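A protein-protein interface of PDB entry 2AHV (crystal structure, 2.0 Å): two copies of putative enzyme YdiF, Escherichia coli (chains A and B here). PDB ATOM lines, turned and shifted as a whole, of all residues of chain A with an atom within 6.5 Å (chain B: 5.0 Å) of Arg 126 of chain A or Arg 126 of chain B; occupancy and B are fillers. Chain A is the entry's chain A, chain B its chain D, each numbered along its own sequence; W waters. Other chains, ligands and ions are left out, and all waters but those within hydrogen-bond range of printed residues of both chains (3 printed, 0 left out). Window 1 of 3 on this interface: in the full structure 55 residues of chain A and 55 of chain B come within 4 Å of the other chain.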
ATOM      1  N   LEU A 121      13.694   1.721 -31.199  1.00  0.00           N
ATOM      2  CA  LEU A 121      14.386   0.503 -30.782  1.00  0.00           C
ATOM      3  C   LEU A 121      13.941   0.056 -29.393  1.00  0.00           C
ATOM      4  O   LEU A 121      13.528  -1.094 -29.207  1.00  0.00           O
ATOM      5  CB  LEU A 121      15.912   0.664 -30.847  1.00  0.00           C
ATOM      6  CG  LEU A 121      16.759  -0.591 -30.568  1.00  0.00           C
ATOM      7  CD1 LEU A 121      16.221  -1.846 -31.262  1.00  0.00           C
ATOM      8  CD2 LEU A 121      18.227  -0.389 -30.930  1.00  0.00           C
ATOM      9  N   THR A 122      13.989   0.960 -28.422  1.00  0.00           N
ATOM     10  CA  THR A 122      13.566   0.592 -27.078  1.00  0.00           C
ATOM     11  C   THR A 122      12.059   0.274 -26.999  1.00  0.00           C
ATOM     12  O   THR A 122      11.660  -0.629 -26.253  1.00  0.00           O
ATOM     13  CB  THR A 122      14.069   1.611 -26.010  1.00  0.00           C
ATOM     14  OG1 THR A 122      13.723   1.131 -24.708  1.00  0.00           O
ATOM     15  CG2 THR A 122      13.364   2.954 -26.111  1.00  0.00           C
ATOM     16  N   GLN A 123      11.242   0.950 -27.810  1.00  0.00           N
ATOM     17  CA  GLN A 123       9.816   0.603 -27.927  1.00  0.00           C
ATOM     18  C   GLN A 123       9.587  -0.802 -28.516  1.00  0.00           C
ATOM     19  O   GLN A 123       8.646  -1.497 -28.106  1.00  0.00           O
ATOM     20  CB  GLN A 123       9.058   1.621 -28.778  1.00  0.00           C
ATOM     21  CG  GLN A 123       8.860   3.000 -28.148  1.00  0.00           C
ATOM     22  CD  GLN A 123       8.341   4.016 -29.144  1.00  0.00           C
ATOM     23  OE1 GLN A 123       8.523   3.855 -30.355  1.00  0.00           O
ATOM     24  NE2 GLN A 123       7.684   5.061 -28.645  1.00  0.00           N
ATOM     25  N   THR A 124      10.422  -1.220 -29.468  1.00  0.00           N
ATOM     26  CA  THR A 124      10.282  -2.570 -30.034  1.00  0.00           C
ATOM     27  C   THR A 124      10.668  -3.652 -29.033  1.00  0.00           C
ATOM     28  O   THR A 124      10.117  -4.746 -29.069  1.00  0.00           O
ATOM     29  CB  THR A 124      11.061  -2.779 -31.348  1.00  0.00           C
ATOM     30  OG1 THR A 124      12.466  -2.552 -31.144  1.00  0.00           O
ATOM     31  CG2 THR A 124      10.596  -1.799 -32.433  1.00  0.00           C
ATOM     32  N   LEU A 125      11.616  -3.350 -28.152  1.00  0.00           N
ATOM     33  CA  LEU A 125      11.967  -4.291 -27.090  1.00  0.00           C
ATOM     34  C   LEU A 125      10.789  -4.441 -26.137  1.00  0.00           C
ATOM     35  O   LEU A 125      10.461  -5.556 -25.719  1.00  0.00           O
ATOM     36  CB  LEU A 125      13.237  -3.856 -26.360  1.00  0.00           C
ATOM     37  CG  LEU A 125      14.524  -4.049 -27.170  1.00  0.00           C
ATOM     38  CD1 LEU A 125      15.661  -3.309 -26.532  1.00  0.00           C
ATOM     39  CD2 LEU A 125      14.880  -5.542 -27.361  1.00  0.00           C
ATOM     40  N   ARG A 126      10.125  -3.322 -25.844  1.00  0.00           N
ATOM     41  CA  ARG A 126       8.914  -3.316 -25.014  1.00  0.00           C
ATOM     42  C   ARG A 126       7.777  -4.095 -25.669  1.00  0.00           C
ATOM     43  O   ARG A 126       7.034  -4.820 -24.997  1.00  0.00           O
ATOM     44  CB  ARG A 126       8.470  -1.874 -24.733  1.00  0.00           C
ATOM     45  CG  ARG A 126       7.398  -1.740 -23.653  1.00  0.00           C
ATOM     46  CD  ARG A 126       7.104  -0.295 -23.269  1.00  0.00           C
ATOM     47  NE  ARG A 126       6.661   0.517 -24.411  1.00  0.00           N
ATOM     48  CZ  ARG A 126       6.544   1.852 -24.392  1.00  0.00           C
ATOM     49  NH1 ARG A 126       6.835   2.529 -23.289  1.00  0.00           N
ATOM     50  NH2 ARG A 126       6.128   2.513 -25.480  1.00  0.00           N
ATOM     51  N   ALA A 127       7.629  -3.923 -26.977  1.00  0.00           N
ATOM     52  CA  ALA A 127       6.690  -4.714 -27.769  1.00  0.00           C
ATOM     53  C   ALA A 127       7.044  -6.210 -27.710  1.00  0.00           C
ATOM     54  O   ALA A 127       6.159  -7.062 -27.627  1.00  0.00           O
ATOM     55  CB  ALA A 127       6.671  -4.221 -29.223  1.00  0.00           C
ATOM     56  N   ALA A 128       8.338  -6.517 -27.760  1.00  0.00           N
ATOM     57  CA  ALA A 128       8.819  -7.901 -27.726  1.00  0.00           C
ATOM     58  C   ALA A 128       8.534  -8.589 -26.387  1.00  0.00           C
ATOM     59  O   ALA A 128       8.245  -9.785 -26.351  1.00  0.00           O
ATOM     60  CB  ALA A 128      10.308  -7.951 -28.055  1.00  0.00           C
ATOM     61  N   ALA A 129       8.615  -7.826 -25.299  1.00  0.00           N
ATOM     62  CA  ALA A 129       8.208  -8.297 -23.976  1.00  0.00           C
ATOM     63  C   ALA A 129       6.759  -8.771 -23.986  1.00  0.00           C
ATOM     64  O   ALA A 129       6.429  -9.774 -23.341  1.00  0.00           O
ATOM     65  CB  ALA A 129       8.384  -7.185 -22.943  1.00  0.00           C
ATOM     66  N   ALA A 130       5.910  -8.033 -24.706  1.00  0.00           N
ATOM     67  CA  ALA A 130       4.491  -8.348 -24.848  1.00  0.00           C
ATOM     68  C   ALA A 130       4.162  -9.348 -25.976  1.00  0.00           C
ATOM     69  O   ALA A 130       2.984  -9.637 -26.216  1.00  0.00           O
ATOM     70  CB  ALA A 130       3.678  -7.052 -25.039  1.00  0.00           C
ATOM     71  N   HIS A 131       5.190  -9.879 -26.641  1.00  0.00           N
ATOM     72  CA  HIS A 131       5.037 -10.761 -27.813  1.00  0.00           C
ATOM     73  C   HIS A 131       4.259 -10.078 -28.952  1.00  0.00           C
ATOM     74  O   HIS A 131       3.568 -10.739 -29.747  1.00  0.00           O
ATOM     75  CB  HIS A 131       4.401 -12.111 -27.424  1.00  0.00           C
ATOM     76  CG  HIS A 131       5.329 -13.037 -26.690  1.00  0.00           C
ATOM     77  ND1 HIS A 131       5.030 -14.366 -26.473  1.00  0.00           N
ATOM     78  CD2 HIS A 131       6.548 -12.831 -26.135  1.00  0.00           C
ATOM     79  CE1 HIS A 131       6.020 -14.934 -25.807  1.00  0.00           C
ATOM     80  NE2 HIS A 131       6.951 -14.024 -25.583  1.00  0.00           N
ATOM     81  N   GLN A 132       4.384  -8.755 -29.045  1.00  0.00           N
ATOM     82  CA  GLN A 132       3.842  -8.037 -30.201  1.00  0.00           C
ATOM     83  C   GLN A 132       4.867  -8.151 -31.316  1.00  0.00           C
ATOM     84  O   GLN A 132       6.063  -8.113 -31.044  1.00  0.00           O
ATOM     85  CB  GLN A 132       3.529  -6.578 -29.860  1.00  0.00           C
ATOM     86  CG  GLN A 132       2.406  -6.426 -28.844  1.00  0.00           C
ATOM     87  CD  GLN A 132       2.231  -4.988 -28.355  1.00  0.00           C
ATOM     88  OE1 GLN A 132       2.829  -4.062 -28.904  1.00  0.00           O
ATOM     89  NE2 GLN A 132       1.406  -4.804 -27.330  1.00  0.00           N
ATOM     90  N   VAL A 210      12.230  -3.019 -19.266  1.00  0.00           N
ATOM     91  CA  VAL A 210      11.849  -3.449 -20.620  1.00  0.00           C
ATOM     92  C   VAL A 210      12.765  -4.584 -21.132  1.00  0.00           C
ATOM     93  O   VAL A 210      12.293  -5.616 -21.621  1.00  0.00           O
ATOM     94  CB  VAL A 210      11.849  -2.228 -21.591  1.00  0.00           C
ATOM     95  CG1 VAL A 210      11.927  -2.660 -23.045  1.00  0.00           C
ATOM     96  CG2 VAL A 210      10.621  -1.351 -21.344  1.00  0.00           C
ATOM     97  N   ILE A 211      14.072  -4.397 -20.999  1.00  0.00           N
ATOM     98  CA  ILE A 211      15.039  -5.388 -21.456  1.00  0.00           C
ATOM     99  C   ILE A 211      14.867  -6.707 -20.682  1.00  0.00           C
ATOM    100  O   ILE A 211      14.894  -7.790 -21.280  1.00  0.00           O
ATOM    101  CB  ILE A 211      16.480  -4.857 -21.299  1.00  0.00           C
ATOM    102  CG1 ILE A 211      16.731  -3.685 -22.262  1.00  0.00           C
ATOM    103  CG2 ILE A 211      17.504  -5.990 -21.542  1.00  0.00           C
ATOM    104  CD1 ILE A 211      18.088  -2.975 -22.054  1.00  0.00           C
ATOM    105  N   GLN A 213      12.171  -7.848 -19.102  1.00  0.00           N
ATOM    106  CA  GLN A 213      10.907  -8.458 -19.519  1.00  0.00           C
ATOM    107  C   GLN A 213      11.008  -9.112 -20.909  1.00  0.00           C
ATOM    108  O   GLN A 213      10.498 -10.216 -21.121  1.00  0.00           O
ATOM    109  CB  GLN A 213       9.790  -7.415 -19.526  1.00  0.00           C
ATOM    110  CG  GLN A 213       9.288  -6.962 -18.133  1.00  0.00           C
ATOM    111  CD  GLN A 213       8.090  -6.013 -18.221  1.00  0.00           C
ATOM    112  OE1 GLN A 213       7.896  -5.348 -19.235  1.00  0.00           O
ATOM    113  NE2 GLN A 213       7.285  -5.961 -17.170  1.00  0.00           N
ATOM    114  N   ALA A 214      11.668  -8.426 -21.847  1.00  0.00           N
ATOM    115  CA  ALA A 214      11.818  -8.906 -23.223  1.00  0.00           C
ATOM    116  C   ALA A 214      12.577 -10.234 -23.277  1.00  0.00           C
ATOM    117  O   ALA A 214      12.147 -11.167 -23.970  1.00  0.00           O
ATOM    118  CB  ALA A 214      12.516  -7.852 -24.087  1.00  0.00           C
ATOM    119  N   ASP A 358      11.878   6.399 -17.002  1.00  0.00           N
ATOM    120  CA  ASP A 358      12.509   5.367 -17.826  1.00  0.00           C
ATOM    121  C   ASP A 358      12.670   5.889 -19.274  1.00  0.00           C
ATOM    122  O   ASP A 358      11.949   6.795 -19.714  1.00  0.00           O
ATOM    123  CB  ASP A 358      11.716   4.056 -17.787  1.00  0.00           C
ATOM    124  CG  ASP A 358      10.403   4.151 -18.519  1.00  0.00           C
ATOM    125  OD1 ASP A 358       9.469   4.770 -17.966  1.00  0.00           O
ATOM    126  OD2 ASP A 358      10.207   3.636 -19.647  1.00  0.00           O
ATOM    127  N   THR A 360      12.158   4.531 -22.319  1.00  0.00           N
ATOM    128  CA  THR A 360      11.097   4.287 -23.300  1.00  0.00           C
ATOM    129  C   THR A 360       9.974   5.324 -23.172  1.00  0.00           C
ATOM    130  O   THR A 360       9.554   5.898 -24.177  1.00  0.00           O
ATOM    131  CB  THR A 360      10.563   2.831 -23.219  1.00  0.00           C
ATOM    132  OG1 THR A 360      11.665   1.923 -23.059  1.00  0.00           O
ATOM    133  CG2 THR A 360       9.938   2.417 -24.548  1.00  0.00           C
ATOM    134  N   SER A 361       9.532   5.597 -21.944  1.00  0.00           N
ATOM    135  CA  SER A 361       8.479   6.592 -21.698  1.00  0.00           C
ATOM    136  C   SER A 361       8.889   7.999 -22.131  1.00  0.00           C
ATOM    137  O   SER A 361       8.042   8.793 -22.547  1.00  0.00           O
ATOM    138  CB  SER A 361       8.083   6.639 -20.223  1.00  0.00           C
ATOM    139  OG  SER A 361       7.622   5.366 -19.805  1.00  0.00           O
ATOM    140  N   ASP A 364       8.336   7.979 -25.845  1.00  0.00           N
ATOM    141  CA  ASP A 364       6.895   8.062 -26.096  1.00  0.00           C
ATOM    142  C   ASP A 364       6.492   9.542 -26.134  1.00  0.00           C
ATOM    143  O   ASP A 364       5.813   9.987 -27.060  1.00  0.00           O
ATOM    144  CB  ASP A 364       6.084   7.351 -24.996  1.00  0.00           C
ATOM    145  CG  ASP A 364       6.266   5.840 -24.986  1.00  0.00           C
ATOM    146  OD1 ASP A 364       6.583   5.250 -26.048  1.00  0.00           O
ATOM    147  OD2 ASP A 364       6.085   5.156 -23.944  1.00  0.00           O
ATOM    148  N   THR B 122      -4.784   0.098 -22.047  1.00  0.00           N
ATOM    149  CA  THR B 122      -3.759   0.990 -21.509  1.00  0.00           C
ATOM    150  C   THR B 122      -2.522   1.070 -22.427  1.00  0.00           C
ATOM    151  O   THR B 122      -1.917   2.133 -22.577  1.00  0.00           O
ATOM    152  CB  THR B 122      -3.426   0.667 -20.028  1.00  0.00           C
ATOM    153  OG1 THR B 122      -2.386   1.549 -19.575  1.00  0.00           O
ATOM    154  CG2 THR B 122      -2.839  -0.749 -19.848  1.00  0.00           C
ATOM    155  N   GLN B 123      -2.188  -0.042 -23.084  1.00  0.00           N
ATOM    156  CA  GLN B 123      -1.188  -0.043 -24.148  1.00  0.00           C
ATOM    157  C   GLN B 123      -1.561   0.894 -25.310  1.00  0.00           C
ATOM    158  O   GLN B 123      -0.674   1.554 -25.874  1.00  0.00           O
ATOM    159  CB  GLN B 123      -0.941  -1.458 -24.679  1.00  0.00           C
ATOM    160  CG  GLN B 123      -0.176  -2.384 -23.735  1.00  0.00           C
ATOM    161  CD  GLN B 123      -0.095  -3.815 -24.252  1.00  0.00           C
ATOM    162  OE1 GLN B 123      -0.882  -4.218 -25.108  1.00  0.00           O
ATOM    163  NE2 GLN B 123       0.858  -4.583 -23.736  1.00  0.00           N
ATOM    164  N   THR B 124      -2.845   0.974 -25.675  1.00  0.00           N
ATOM    165  CA  THR B 124      -3.229   1.859 -26.802  1.00  0.00           C
ATOM    166  C   THR B 124      -3.126   3.334 -26.406  1.00  0.00           C
ATOM    167  O   THR B 124      -2.886   4.184 -27.250  1.00  0.00           O
ATOM    168  CB  THR B 124      -4.639   1.551 -27.422  1.00  0.00           C
ATOM    169  OG1 THR B 124      -5.653   1.631 -26.417  1.00  0.00           O
ATOM    170  CG2 THR B 124      -4.725   0.123 -27.964  1.00  0.00           C
ATOM    171  N   LEU B 125      -3.309   3.629 -25.123  1.00  0.00           N
ATOM    172  CA  LEU B 125      -3.147   5.004 -24.623  1.00  0.00           C
ATOM    173  C   LEU B 125      -1.677   5.414 -24.632  1.00  0.00           C
ATOM    174  O   LEU B 125      -1.348   6.564 -24.892  1.00  0.00           O
ATOM    175  CB  LEU B 125      -3.747   5.149 -23.221  1.00  0.00           C
ATOM    176  CG  LEU B 125      -5.278   5.120 -23.193  1.00  0.00           C
ATOM    177  CD1 LEU B 125      -5.801   4.892 -21.796  1.00  0.00           C
ATOM    178  CD2 LEU B 125      -5.844   6.431 -23.770  1.00  0.00           C
ATOM    179  N   ARG B 126      -0.801   4.452 -24.379  1.00  0.00           N
ATOM    180  CA  ARG B 126       0.629   4.683 -24.430  1.00  0.00           C
ATOM    181  C   ARG B 126       1.057   4.880 -25.884  1.00  0.00           C
ATOM    182  O   ARG B 126       1.932   5.712 -26.168  1.00  0.00           O
ATOM    183  CB  ARG B 126       1.369   3.520 -23.758  1.00  0.00           C
ATOM    184  CG  ARG B 126       2.855   3.731 -23.521  1.00  0.00           C
ATOM    185  CD  ARG B 126       3.499   2.596 -22.736  1.00  0.00           C
ATOM    186  NE  ARG B 126       3.338   1.324 -23.437  1.00  0.00           N
ATOM    187  CZ  ARG B 126       3.615   0.127 -22.924  1.00  0.00           C
ATOM    188  NH1 ARG B 126       4.088   0.004 -21.678  1.00  0.00           N
ATOM    189  NH2 ARG B 126       3.427  -0.958 -23.676  1.00  0.00           N
ATOM    190  N   ALA B 127       0.428   4.139 -26.802  1.00  0.00           N
ATOM    191  CA  ALA B 127       0.655   4.331 -28.235  1.00  0.00           C
ATOM    192  C   ALA B 127       0.195   5.726 -28.648  1.00  0.00           C
ATOM    193  O   ALA B 127       0.919   6.440 -29.346  1.00  0.00           O
ATOM    194  CB  ALA B 127      -0.085   3.272 -29.053  1.00  0.00           C
ATOM    195  N   ALA B 128      -1.004   6.104 -28.210  1.00  0.00           N
ATOM    196  CA  ALA B 128      -1.568   7.443 -28.498  1.00  0.00           C
ATOM    197  C   ALA B 128      -0.669   8.588 -28.019  1.00  0.00           C
ATOM    198  O   ALA B 128      -0.541   9.602 -28.715  1.00  0.00           O
ATOM    199  CB  ALA B 128      -2.993   7.582 -27.912  1.00  0.00           C
ATOM    200  N   ALA B 129      -0.034   8.414 -26.859  1.00  0.00           N
ATOM    201  CA  ALA B 129       0.989   9.351 -26.371  1.00  0.00           C
ATOM    202  C   ALA B 129       2.081   9.567 -27.408  1.00  0.00           C
ATOM    203  O   ALA B 129       2.538  10.698 -27.599  1.00  0.00           O
ATOM    204  CB  ALA B 129       1.614   8.870 -25.053  1.00  0.00           C
ATOM    205  N   ALA B 130       2.471   8.487 -28.081  1.00  0.00           N
ATOM    206  CA  ALA B 130       3.527   8.538 -29.083  1.00  0.00           C
ATOM    207  C   ALA B 130       3.014   8.805 -30.509  1.00  0.00           C
ATOM    208  O   ALA B 130       3.796   8.746 -31.458  1.00  0.00           O
ATOM    209  CB  ALA B 130       4.366   7.239 -29.051  1.00  0.00           C
ATOM    210  N   VAL B 210       1.101   7.497 -18.349  1.00  0.00           N
ATOM    211  CA  VAL B 210       0.611   7.181 -19.684  1.00  0.00           C
ATOM    212  C   VAL B 210      -0.602   8.030 -20.076  1.00  0.00           C
ATOM    213  O   VAL B 210      -0.667   8.549 -21.198  1.00  0.00           O
ATOM    214  CB  VAL B 210       0.288   5.670 -19.799  1.00  0.00           C
ATOM    215  CG1 VAL B 210      -0.662   5.390 -20.959  1.00  0.00           C
ATOM    216  CG2 VAL B 210       1.575   4.886 -19.934  1.00  0.00           C
ATOM    217  N   THR B 360       0.576  -0.582 -17.161  1.00  0.00           N
ATOM    218  CA  THR B 360       0.904  -0.947 -18.540  1.00  0.00           C
ATOM    219  C   THR B 360       2.045  -1.965 -18.618  1.00  0.00           C
ATOM    220  O   THR B 360       1.918  -2.970 -19.316  1.00  0.00           O
ATOM    221  CB  THR B 360       1.194   0.296 -19.429  1.00  0.00           C
ATOM    222  OG1 THR B 360       0.301   1.362 -19.079  1.00  0.00           O
ATOM    223  CG2 THR B 360       0.823  -0.018 -20.907  1.00  0.00           C
ATOM    224  N   SER B 361       3.137  -1.710 -17.893  1.00  0.00           N
ATOM    225  CA  SER B 361       4.276  -2.627 -17.813  1.00  0.00           C
ATOM    226  C   SER B 361       3.873  -4.005 -17.257  1.00  0.00           C
ATOM    227  O   SER B 361       4.394  -5.029 -17.691  1.00  0.00           O
ATOM    228  CB  SER B 361       5.384  -2.022 -16.950  1.00  0.00           C
ATOM    229  OG  SER B 361       5.746  -0.733 -17.447  1.00  0.00           O
ATOM    230  N   ASP B 364       2.285  -5.783 -20.197  1.00  0.00           N
ATOM    231  CA  ASP B 364       3.319  -6.215 -21.139  1.00  0.00           C
ATOM    232  C   ASP B 364       3.873  -7.569 -20.694  1.00  0.00           C
ATOM    233  O   ASP B 364       4.075  -8.475 -21.511  1.00  0.00           O
ATOM    234  CB  ASP B 364       4.495  -5.222 -21.178  1.00  0.00           C
ATOM    235  CG  ASP B 364       4.126  -3.837 -21.730  1.00  0.00           C
ATOM    236  OD1 ASP B 364       3.230  -3.707 -22.606  1.00  0.00           O
ATOM    237  OD2 ASP B 364       4.732  -2.804 -21.341  1.00  0.00           O
HETATM  238  O   HOH W   1       7.438  -2.910 -20.084  1.00  0.00           O
HETATM  239  O   HOH W   2       4.074   4.440 -27.122  1.00  0.00           O
HETATM  240  O   HOH W   3       4.495  -3.863 -25.037  1.00  0.00           O
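NE2 of Gln 123 of chain A touches CB of Ala 130 of chain B, 3.99 Å away. CD of Arg 126 of chain B touches NH1 of Arg 126 of chain A, 3.4 Å away. Asp 364 of chain B touches Arg 126 of chain A. Ala 130 of chain A touches Gln 123 of chain B (CB to NE2, 3.97 Å). Ala 130 of chain A touches Asp 364 of chain B. Gln 213 of chain A touches Asp 364 of chain B (OE1 to CB, 3.9 Å). Arg 126 of chain B touches Asp 364 of chain A. O of Asp 364 of chain A touches CA of Ala 130 of chain B, 3.4 Å away.
The side-chain amide oxygen of Gln 123 of chain B sits at hydrogen-bond distance from the side-chain amide nitrogen of Gln 132 of chain A (3.2 Å). The side-chain amide nitrogen (NE2) of Gln 213 of chain A sits at hydrogen-bond distance from the backbone carbonyl oxygen (O) of Ser 361 of chain B (3.1 Å). The backbone carbonyl oxygen of Asp 364 of chain B sits close to the backbone carbonyl oxygen of Ala 129 of chain A (3.3 Å). O of Asp 364 of chain A sits close to O of Ala 129 of chain B.
The side-chain carboxylate (OD1) of Asp 364 of chain A sits at hydrogen-bond distance from the side-chain amide nitrogen (NE2) of Gln 123 of chain A, 2.8 Å away. NH1 of Arg 126 of chain B lies within salt-bridge range of OD2 of Asp 364 of chain B (2.9 Å). The side-chain carboxylate (OD2) of Asp 364 of chain A is in salt-bridge range of the guanidinium group (NH1) of Arg 126 of chain A, 2.8 Å away. The side-chain amide nitrogen of Gln 123 of chain B lies within hydrogen-bond range of the side-chain carboxylate of Asp 364 of chain B, 2.8 Å away. The backbone NH (N) of Gln 132 of chain A is in hydrogen-bond range of the backbone carbonyl oxygen (O) of Ala 127 of chain A (2.8 Å).
Water W1 bridges OE1 of Gln 213 of chain A and OD2 of Asp 364 of chain B. Water W2 lies within hydrogen-bond range of the backbone carbonyl oxygen of Arg 126 of chain B (2.7 Å), the side-chain carboxylate of Asp 364 of chain A (2.8 Å) and the guanidinium group of Arg 126 of chain A (3.3 Å). Water W3 lies within hydrogen-bond range of the backbone carbonyl oxygen (O) of Arg 126 of chain A (2.7 Å), the side-chain carboxylate (OD1) of Asp 364 of chain B (2.7 Å) and the guanidinium group (NH2) of Arg 126 of chain B (3.4 Å).
Of chain B, only Arg 126 and Asp 364 come within 4 Å of Arg 126 of chain A. Of chain A, only Arg 126 and Asp 364 come within 4 Å of Arg 126 of chain B. Of the printed residues of chain B, Gln 123 of chain A touches Ala 130 (3.99 Å). Of the printed residues of chain A, Gln 123 of chain B touches Ala 130 (3.97 Å) and Gln 132 (3.2 Å). Thr 360 of chain B touches none of the printed residues of chain A. Thr 124 of chain A touches none of the printed residues of chain B. The nearest printed residue of chain B that does not touch Arg 126 of chain A is Ser 361 of chain B (6.0 Å). The nearest residue of chain A that does not touch Arg 126 of chain B is Gln 132 of chain A (5.7 Å).
Arg 126 of chain B touches its own counterpart, Arg 126 of chain A. Arg 126 of chain A touches Asp 364 of chain B, and with the chains exchanged Asp 364 of chain A touches Arg 126 of chain B. Ala 129 of chain A touches Asp 364 of chain B, and with the chains exchanged Asp 364 of chain A touches Ala 129 of chain B. Ala 130 of chain A touches Asp 364 of chain B, and with the chains exchanged Asp 364 of chain A touches Ala 130 of chain B. Of the 12 pairs that touch across the chains among the printed residues, 9 have their exchanged pair printed and touching as well.
Printed residues of chain A that touch a printed residue of chain B: Gln 123, Arg 126, Ala 129, Ala 130, Gln 132, Gln 213 and Asp 364. Hydrophobic or aromatic side chains of chain A within 4 Å of the printed part of chain B: Ala 130. Among the printed residues, no Asp or Glu carboxylate lies within 4 Å of a Lys or Arg side-chain nitrogen of the other chain.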
